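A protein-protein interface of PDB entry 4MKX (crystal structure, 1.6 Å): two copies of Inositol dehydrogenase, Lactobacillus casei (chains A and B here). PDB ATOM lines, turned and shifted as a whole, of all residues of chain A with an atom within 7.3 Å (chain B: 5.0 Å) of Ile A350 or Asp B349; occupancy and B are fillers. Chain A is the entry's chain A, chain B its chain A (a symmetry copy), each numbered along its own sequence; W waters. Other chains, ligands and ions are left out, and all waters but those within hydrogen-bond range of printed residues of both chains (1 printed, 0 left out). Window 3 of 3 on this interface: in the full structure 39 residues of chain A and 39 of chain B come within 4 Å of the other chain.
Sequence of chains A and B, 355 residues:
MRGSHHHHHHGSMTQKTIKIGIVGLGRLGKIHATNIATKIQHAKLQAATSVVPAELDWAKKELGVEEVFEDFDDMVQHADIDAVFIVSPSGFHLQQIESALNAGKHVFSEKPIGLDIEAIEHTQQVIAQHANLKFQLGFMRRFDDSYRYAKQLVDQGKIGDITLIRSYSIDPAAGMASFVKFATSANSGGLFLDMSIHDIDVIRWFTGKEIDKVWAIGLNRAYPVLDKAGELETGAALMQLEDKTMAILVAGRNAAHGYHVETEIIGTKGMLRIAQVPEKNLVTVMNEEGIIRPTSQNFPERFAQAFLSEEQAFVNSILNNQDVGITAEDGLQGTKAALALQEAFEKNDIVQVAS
The side-chain amide oxygen of Gln A240 sits at hydrogen-bond distance from the side-chain amide nitrogen of Asn B348, 3.1 Å away.
O of Ala B344 lies within hydrogen-bond range of N of Asp B349.
The backbone carbonyl oxygen (O) of Lys A213 is in hydrogen-bond range of the backbone NH (N) of Gln A240 (2.9 Å).
The backbone carbonyl oxygen of Ala A344 lies within hydrogen-bond range of the backbone NH of Asp A349 (3.3 Å).
The backbone NH (N) of Asp A212 sits at hydrogen-bond distance from the backbone carbonyl oxygen (O) of Gln A240.
N of Leu A238 sits at hydrogen-bond distance from O of Trp A215, 3.0 Å away.
The side-chain amide oxygen (OD1) of Asn A348 lies within hydrogen-bond range of the indole nitrogen (NE1) of Trp A215, at 2.8 Å.
Among the printed residues, merely in contact across the chains: Trp A215 with Trp B215, Trp A215 with Ile B350, Leu A238 with Trp B215, Asp A349 with Ile B350, Ile A350 with Trp B215, Ile A350 with Asp B349 and Ile A350 with Ile B350.
Of the printed residues of chain B, Ile A350 touches Trp B215 (3.6 Å), Asp B349 (3.7 Å) and Ile B350 (3.97 Å).
Of the printed residues of chain A, Trp B215 touches Trp A215, Leu A238 and Ile A350.
Asp B349 touches just one residue of chain A: Ile A350 (3.7 Å).
Of the printed residues of chain A, Ile B350 touches Trp A215 (3.6 Å), Asp A349 (3.7 Å) and Ile A350 (3.97 Å).
The nearest printed residue of chain B that does not touch Ile A350 is Asn B348 (4.01 Å).
Trp B215 touches its own counterpart, Trp A215.
Trp A215 touches Ile B350, and with the chains exchanged Ile A350 touches Trp B215.
Asp A349 touches Ile B350, and with the chains exchanged Ile A350 touches Asp B349.
Ile A350 touches its own counterpart, Ile B350.
Positions printed for both chains: 214, 215, 344, 347, 348, 349, 350 and 351.
Of the 8 pairs that touch across the chains among the printed residues, 6 have their exchanged pair printed and touching as well.
Water W1 bridges the side-chain amino group of Lys A213 and the backbone carbonyl oxygen of Asn B348.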
ATOM      1  N   ASP A 212      -8.246  -4.038  17.588  1.00  0.00           N
ATOM      2  CA  ASP A 212      -9.292  -4.865  16.981  1.00  0.00           C
ATOM      3  C   ASP A 212      -8.803  -6.270  16.662  1.00  0.00           C
ATOM      4  O   ASP A 212      -9.292  -7.247  17.216  1.00  0.00           O
ATOM      5  CB  ASP A 212      -9.841  -4.201  15.719  1.00  0.00           C
ATOM      6  CG  ASP A 212     -11.019  -4.962  15.121  1.00  0.00           C
ATOM      7  OD1 ASP A 212     -11.748  -5.629  15.886  1.00  0.00           O
ATOM      8  OD2 ASP A 212     -11.213  -4.886  13.895  1.00  0.00           O
ATOM      9  N   LYS A 213      -7.839  -6.389  15.753  1.00  0.00           N
ATOM     10  CA  LYS A 213      -7.340  -7.714  15.431  1.00  0.00           C
ATOM     11  C   LYS A 213      -5.826  -7.741  15.342  1.00  0.00           C
ATOM     12  O   LYS A 213      -5.203  -6.716  15.079  1.00  0.00           O
ATOM     13  CB  LYS A 213      -7.981  -8.265  14.156  1.00  0.00           C
ATOM     14  CG  LYS A 213      -7.866  -7.364  12.960  1.00  0.00           C
ATOM     15  CD  LYS A 213      -8.596  -7.975  11.759  1.00  0.00           C
ATOM     16  CE  LYS A 213     -10.096  -7.875  11.921  1.00  0.00           C
ATOM     17  NZ  LYS A 213     -10.827  -8.619  10.856  1.00  0.00           N
ATOM     18  N   VAL A 214      -5.259  -8.911  15.601  1.00  0.00           N
ATOM     19  CA  VAL A 214      -3.815  -9.074  15.708  1.00  0.00           C
ATOM     20  C   VAL A 214      -3.351 -10.359  15.037  1.00  0.00           C
ATOM     21  O   VAL A 214      -4.102 -11.335  14.919  1.00  0.00           O
ATOM     22  CB  VAL A 214      -3.364  -9.134  17.189  1.00  0.00           C
ATOM     23  CG1 VAL A 214      -3.842  -7.910  17.953  1.00  0.00           C
ATOM     24  CG2 VAL A 214      -3.880 -10.393  17.861  1.00  0.00           C
ATOM     25  N   TRP A 215      -2.106 -10.351  14.577  1.00  0.00           N
ATOM     26  CA  TRP A 215      -1.424 -11.573  14.181  1.00  0.00           C
ATOM     27  C   TRP A 215      -0.058 -11.478  14.829  1.00  0.00           C
ATOM     28  O   TRP A 215       0.519 -10.398  14.882  1.00  0.00           O
ATOM     29  CB  TRP A 215      -1.291 -11.665  12.653  1.00  0.00           C
ATOM     30  CG  TRP A 215      -0.616 -12.924  12.163  1.00  0.00           C
ATOM     31  CD1 TRP A 215      -0.758 -14.189  12.668  1.00  0.00           C
ATOM     32  CD2 TRP A 215       0.301 -13.032  11.067  1.00  0.00           C
ATOM     33  NE1 TRP A 215       0.014 -15.072  11.951  1.00  0.00           N
ATOM     34  CE2 TRP A 215       0.688 -14.386  10.974  1.00  0.00           C
ATOM     35  CE3 TRP A 215       0.844 -12.111  10.167  1.00  0.00           C
ATOM     36  CZ2 TRP A 215       1.576 -14.845   9.997  1.00  0.00           C
ATOM     37  CZ3 TRP A 215       1.730 -12.566   9.197  1.00  0.00           C
ATOM     38  CH2 TRP A 215       2.088 -13.924   9.121  1.00  0.00           C
ATOM     39  N   ALA A 216       0.441 -12.590  15.348  1.00  0.00           N
ATOM     40  CA  ALA A 216       1.738 -12.609  16.001  1.00  0.00           C
ATOM     41  C   ALA A 216       2.498 -13.840  15.560  1.00  0.00           C
ATOM     42  O   ALA A 216       1.922 -14.934  15.393  1.00  0.00           O
ATOM     43  CB  ALA A 216       1.597 -12.578  17.526  1.00  0.00           C
ATOM     44  N   LEU A 238       1.561  -7.639  14.363  1.00  0.00           N
ATOM     45  CA  LEU A 238       0.944  -6.535  13.659  1.00  0.00           C
ATOM     46  C   LEU A 238      -0.487  -6.438  14.171  1.00  0.00           C
ATOM     47  O   LEU A 238      -1.152  -7.452  14.350  1.00  0.00           O
ATOM     48  CB  LEU A 238       0.945  -6.802  12.157  1.00  0.00           C
ATOM     49  CG  LEU A 238       0.353  -5.729  11.257  1.00  0.00           C
ATOM     50  CD1 LEU A 238       1.111  -4.413  11.398  1.00  0.00           C
ATOM     51  CD2 LEU A 238       0.387  -6.253   9.818  1.00  0.00           C
ATOM     52  N   GLN A 240      -4.288  -4.154  14.110  1.00  0.00           N
ATOM     53  CA  GLN A 240      -5.119  -3.158  13.487  1.00  0.00           C
ATOM     54  C   GLN A 240      -6.040  -2.674  14.588  1.00  0.00           C
ATOM     55  O   GLN A 240      -6.686  -3.484  15.257  1.00  0.00           O
ATOM     56  CB  GLN A 240      -5.946  -3.814  12.395  1.00  0.00           C
ATOM     57  CG  GLN A 240      -6.731  -2.856  11.539  1.00  0.00           C
ATOM     58  CD  GLN A 240      -7.247  -3.561  10.289  1.00  0.00           C
ATOM     59  OE1 GLN A 240      -7.866  -4.624  10.380  1.00  0.00           O
ATOM     60  NE2 GLN A 240      -6.967  -2.994   9.129  1.00  0.00           N
ATOM     61  N   ALA A 340      -4.791 -12.270  23.326  1.00  0.00           N
ATOM     62  CA  ALA A 340      -5.087 -12.342  21.903  1.00  0.00           C
ATOM     63  C   ALA A 340      -3.817 -12.537  21.092  1.00  0.00           C
ATOM     64  O   ALA A 340      -3.818 -13.288  20.117  1.00  0.00           O
ATOM     65  CB  ALA A 340      -5.823 -11.099  21.450  1.00  0.00           C
ATOM     66  N   GLU A 343      -2.745 -16.101  21.530  1.00  0.00           N
ATOM     67  CA  GLU A 343      -3.607 -17.021  20.797  1.00  0.00           C
ATOM     68  C   GLU A 343      -3.283 -16.968  19.309  1.00  0.00           C
ATOM     69  O   GLU A 343      -3.237 -17.999  18.641  1.00  0.00           O
ATOM     70  CB  GLU A 343      -5.080 -16.688  21.022  1.00  0.00           C
ATOM     71  CG  GLU A 343      -6.017 -17.752  20.461  1.00  0.00           C
ATOM     72  CD  GLU A 343      -7.473 -17.363  20.564  1.00  0.00           C
ATOM     73  OE1 GLU A 343      -7.790 -16.434  21.344  1.00  0.00           O
ATOM     74  OE2 GLU A 343      -8.298 -17.985  19.857  1.00  0.00           O
ATOM     75  N   ALA A 344      -3.061 -15.761  18.798  1.00  0.00           N
ATOM     76  CA  ALA A 344      -2.682 -15.583  17.401  1.00  0.00           C
ATOM     77  C   ALA A 344      -1.377 -16.300  17.098  1.00  0.00           C
ATOM     78  O   ALA A 344      -1.214 -16.884  16.031  1.00  0.00           O
ATOM     79  CB  ALA A 344      -2.578 -14.105  17.063  1.00  0.00           C
ATOM     80  N   LYS A 347      -2.067 -20.249  17.115  1.00  0.00           N
ATOM     81  CA  LYS A 347      -2.871 -20.650  15.964  1.00  0.00           C
ATOM     82  C   LYS A 347      -2.195 -20.292  14.651  1.00  0.00           C
ATOM     83  O   LYS A 347      -2.547 -20.833  13.602  1.00  0.00           O
ATOM     84  CB  LYS A 347      -4.241 -19.970  16.008  1.00  0.00           C
ATOM     85  CG  LYS A 347      -5.154 -20.468  17.125  1.00  0.00           C
ATOM     86  CD  LYS A 347      -6.524 -19.800  17.055  1.00  0.00           C
ATOM     87  CE  LYS A 347      -7.588 -20.683  17.687  1.00  0.00           C
ATOM     88  NZ  LYS A 347      -7.228 -21.057  19.088  1.00  0.00           N
ATOM     89  N   ASN A 348      -1.220 -19.386  14.719  1.00  0.00           N
ATOM     90  CA  ASN A 348      -0.661 -18.736  13.525  1.00  0.00           C
ATOM     91  C   ASN A 348      -1.771 -18.219  12.600  1.00  0.00           C
ATOM     92  O   ASN A 348      -1.827 -18.565  11.411  1.00  0.00           O
ATOM     93  CB  ASN A 348       0.329 -19.651  12.779  1.00  0.00           C
ATOM     94  CG  ASN A 348       1.270 -18.875  11.854  1.00  0.00           C
ATOM     95  OD1 ASN A 348       1.105 -17.674  11.649  1.00  0.00           O
ATOM     96  ND2 ASN A 348       2.250 -19.565  11.283  1.00  0.00           N
ATOM     97  N   ASP A 349      -2.650 -17.391  13.157  1.00  0.00           N
ATOM     98  CA  ASP A 349      -3.757 -16.807  12.414  1.00  0.00           C
ATOM     99  C   ASP A 349      -4.182 -15.492  13.054  1.00  0.00           C
ATOM    100  O   ASP A 349      -3.804 -15.189  14.191  1.00  0.00           O
ATOM    101  CB  ASP A 349      -4.935 -17.795  12.390  1.00  0.00           C
ATOM    102  CG  ASP A 349      -5.962 -17.470  11.315  1.00  0.00           C
ATOM    103  OD1 ASP A 349      -5.664 -16.667  10.407  1.00  0.00           O
ATOM    104  OD2 ASP A 349      -7.075 -18.038  11.371  1.00  0.00           O
ATOM    105  N   ILE A 350      -4.959 -14.706  12.321  1.00  0.00           N
ATOM    106  CA  ILE A 350      -5.475 -13.443  12.828  1.00  0.00           C
ATOM    107  C   ILE A 350      -6.527 -13.716  13.904  1.00  0.00           C
ATOM    108  O   ILE A 350      -7.413 -14.556  13.721  1.00  0.00           O
ATOM    109  CB  ILE A 350      -6.069 -12.601  11.684  1.00  0.00           C
ATOM    110  CG1 ILE A 350      -4.962 -12.165  10.716  1.00  0.00           C
ATOM    111  CG2 ILE A 350      -6.761 -11.372  12.217  1.00  0.00           C
ATOM    112  CD1 ILE A 350      -5.494 -11.757   9.364  1.00  0.00           C
ATOM    113  N   VAL A 351      -6.408 -13.032  15.035  1.00  0.00           N
ATOM    114  CA  VAL A 351      -7.364 -13.189  16.133  1.00  0.00           C
ATOM    115  C   VAL A 351      -8.025 -11.845  16.428  1.00  0.00           C
ATOM    116  O   VAL A 351      -7.351 -10.815  16.448  1.00  0.00           O
ATOM    117  CB  VAL A 351      -6.658 -13.730  17.375  1.00  0.00           C
ATOM    118  CG1 VAL A 351      -7.588 -13.709  18.587  1.00  0.00           C
ATOM    119  CG2 VAL A 351      -6.167 -15.134  17.116  1.00  0.00           C
ATOM    120  N   GLN A 352      -9.344 -11.843  16.648  1.00  0.00           N
ATOM    121  CA  GLN A 352     -10.047 -10.625  17.041  1.00  0.00           C
ATOM    122  C   GLN A 352     -10.008 -10.535  18.556  1.00  0.00           C
ATOM    123  O   GLN A 352     -10.338 -11.502  19.240  1.00  0.00           O
ATOM    124  CB  GLN A 352     -11.501 -10.628  16.550  1.00  0.00           C
ATOM    125  CG  GLN A 352     -11.645 -10.630  15.025  1.00  0.00           C
ATOM    126  CD  GLN A 352     -12.580  -9.540  14.513  1.00  0.00           C
ATOM    127  OE1 GLN A 352     -12.577  -8.414  15.014  1.00  0.00           O
ATOM    128  NE2 GLN A 352     -13.389  -9.876  13.513  1.00  0.00           N
ATOM    129  N   VAL B 214       2.224 -13.678   4.483  1.00  0.00           N
ATOM    130  CA  VAL B 214       2.188 -12.253   4.782  1.00  0.00           C
ATOM    131  C   VAL B 214       0.790 -11.806   5.183  1.00  0.00           C
ATOM    132  O   VAL B 214      -0.218 -12.407   4.794  1.00  0.00           O
ATOM    133  CB  VAL B 214       2.611 -11.409   3.553  1.00  0.00           C
ATOM    134  CG1 VAL B 214       3.980 -11.835   3.046  1.00  0.00           C
ATOM    135  CG2 VAL B 214       1.590 -11.529   2.437  1.00  0.00           C
ATOM    136  N   TRP B 215       0.731 -10.750   5.985  1.00  0.00           N
ATOM    137  CA  TRP B 215      -0.510 -10.029   6.220  1.00  0.00           C
ATOM    138  C   TRP B 215      -0.140  -8.568   6.073  1.00  0.00           C
ATOM    139  O   TRP B 215       0.937  -8.166   6.497  1.00  0.00           O
ATOM    140  CB  TRP B 215      -1.056 -10.308   7.629  1.00  0.00           C
ATOM    141  CG  TRP B 215      -2.363  -9.615   7.936  1.00  0.00           C
ATOM    142  CD1 TRP B 215      -3.419  -9.424   7.086  1.00  0.00           C
ATOM    143  CD2 TRP B 215      -2.746  -9.028   9.187  1.00  0.00           C
ATOM    144  NE1 TRP B 215      -4.431  -8.756   7.733  1.00  0.00           N
ATOM    145  CE2 TRP B 215      -4.037  -8.485   9.019  1.00  0.00           C
ATOM    146  CE3 TRP B 215      -2.113  -8.895  10.426  1.00  0.00           C
ATOM    147  CZ2 TRP B 215      -4.719  -7.842  10.055  1.00  0.00           C
ATOM    148  CZ3 TRP B 215      -2.789  -8.252  11.457  1.00  0.00           C
ATOM    149  CH2 TRP B 215      -4.081  -7.732  11.263  1.00  0.00           C
ATOM    150  N   ALA B 344      -3.175  -9.698   0.361  1.00  0.00           N
ATOM    151  CA  ALA B 344      -3.410  -9.747   1.800  1.00  0.00           C
ATOM    152  C   ALA B 344      -4.107  -8.484   2.279  1.00  0.00           C
ATOM    153  O   ALA B 344      -4.978  -8.536   3.141  1.00  0.00           O
ATOM    154  CB  ALA B 344      -2.104  -9.960   2.545  1.00  0.00           C
ATOM    155  N   LYS B 347      -7.895  -8.550   0.969  1.00  0.00           N
ATOM    156  CA  LYS B 347      -8.676  -9.570   1.662  1.00  0.00           C
ATOM    157  C   LYS B 347      -8.697  -9.341   3.164  1.00  0.00           C
ATOM    158  O   LYS B 347      -9.554  -9.883   3.865  1.00  0.00           O
ATOM    159  CB  LYS B 347      -8.099 -10.961   1.390  1.00  0.00           C
ATOM    160  CG  LYS B 347      -8.285 -11.448  -0.044  1.00  0.00           C
ATOM    161  CD  LYS B 347      -7.754 -12.868  -0.216  1.00  0.00           C
ATOM    162  CE  LYS B 347      -8.463 -13.575  -1.360  1.00  0.00           C
ATOM    163  NZ  LYS B 347      -8.368 -12.793  -2.630  1.00  0.00           N
ATOM    164  N   ASN B 348      -7.757  -8.530   3.650  1.00  0.00           N
ATOM    165  CA  ASN B 348      -7.471  -8.423   5.088  1.00  0.00           C
ATOM    166  C   ASN B 348      -7.329  -9.808   5.733  1.00  0.00           C
ATOM    167  O   ASN B 348      -8.025 -10.136   6.704  1.00  0.00           O
ATOM    168  CB  ASN B 348      -8.510  -7.551   5.819  1.00  0.00           C
ATOM    169  CG  ASN B 348      -7.999  -7.025   7.163  1.00  0.00           C
ATOM    170  OD1 ASN B 348      -6.930  -7.417   7.629  1.00  0.00           O
ATOM    171  ND2 ASN B 348      -8.770  -6.149   7.795  1.00  0.00           N
ATOM    172  N   ASP B 349      -6.425 -10.614   5.183  1.00  0.00           N
ATOM    173  CA  ASP B 349      -6.164 -11.955   5.681  1.00  0.00           C
ATOM    174  C   ASP B 349      -4.744 -12.378   5.330  1.00  0.00           C
ATOM    175  O   ASP B 349      -4.086 -11.753   4.491  1.00  0.00           O
ATOM    176  CB  ASP B 349      -7.180 -12.935   5.072  1.00  0.00           C
ATOM    177  CG  ASP B 349      -7.262 -14.253   5.828  1.00  0.00           C
ATOM    178  OD1 ASP B 349      -6.759 -14.338   6.966  1.00  0.00           O
ATOM    179  OD2 ASP B 349      -7.852 -15.212   5.280  1.00  0.00           O
ATOM    180  N   ILE B 350      -4.268 -13.434   5.975  1.00  0.00           N
ATOM    181  CA  ILE B 350      -2.944 -13.973   5.701  1.00  0.00           C
ATOM    182  C   ILE B 350      -2.937 -14.637   4.324  1.00  0.00           C
ATOM    183  O   ILE B 350      -3.844 -15.404   3.989  1.00  0.00           O
ATOM    184  CB  ILE B 350      -2.529 -14.975   6.794  1.00  0.00           C
ATOM    185  CG1 ILE B 350      -2.345 -14.253   8.134  1.00  0.00           C
ATOM    186  CG2 ILE B 350      -1.239 -15.669   6.433  1.00  0.00           C
ATOM    187  CD1 ILE B 350      -2.402 -15.190   9.317  1.00  0.00           C
ATOM    188  N   VAL B 351      -1.933 -14.315   3.516  1.00  0.00           N
ATOM    189  CA  VAL B 351      -1.805 -14.899   2.180  1.00  0.00           C
ATOM    190  C   VAL B 351      -0.477 -15.645   2.077  1.00  0.00           C
ATOM    191  O   VAL B 351       0.549 -15.152   2.548  1.00  0.00           O
ATOM    192  CB  VAL B 351      -1.896 -13.807   1.115  1.00  0.00           C
ATOM    193  CG1 VAL B 351      -1.562 -14.361  -0.269  1.00  0.00           C
ATOM    194  CG2 VAL B 351      -3.280 -13.204   1.117  1.00  0.00           C
HETATM  195  O   HOH W   1      -9.182  -9.897   9.164  1.00  0.00           O
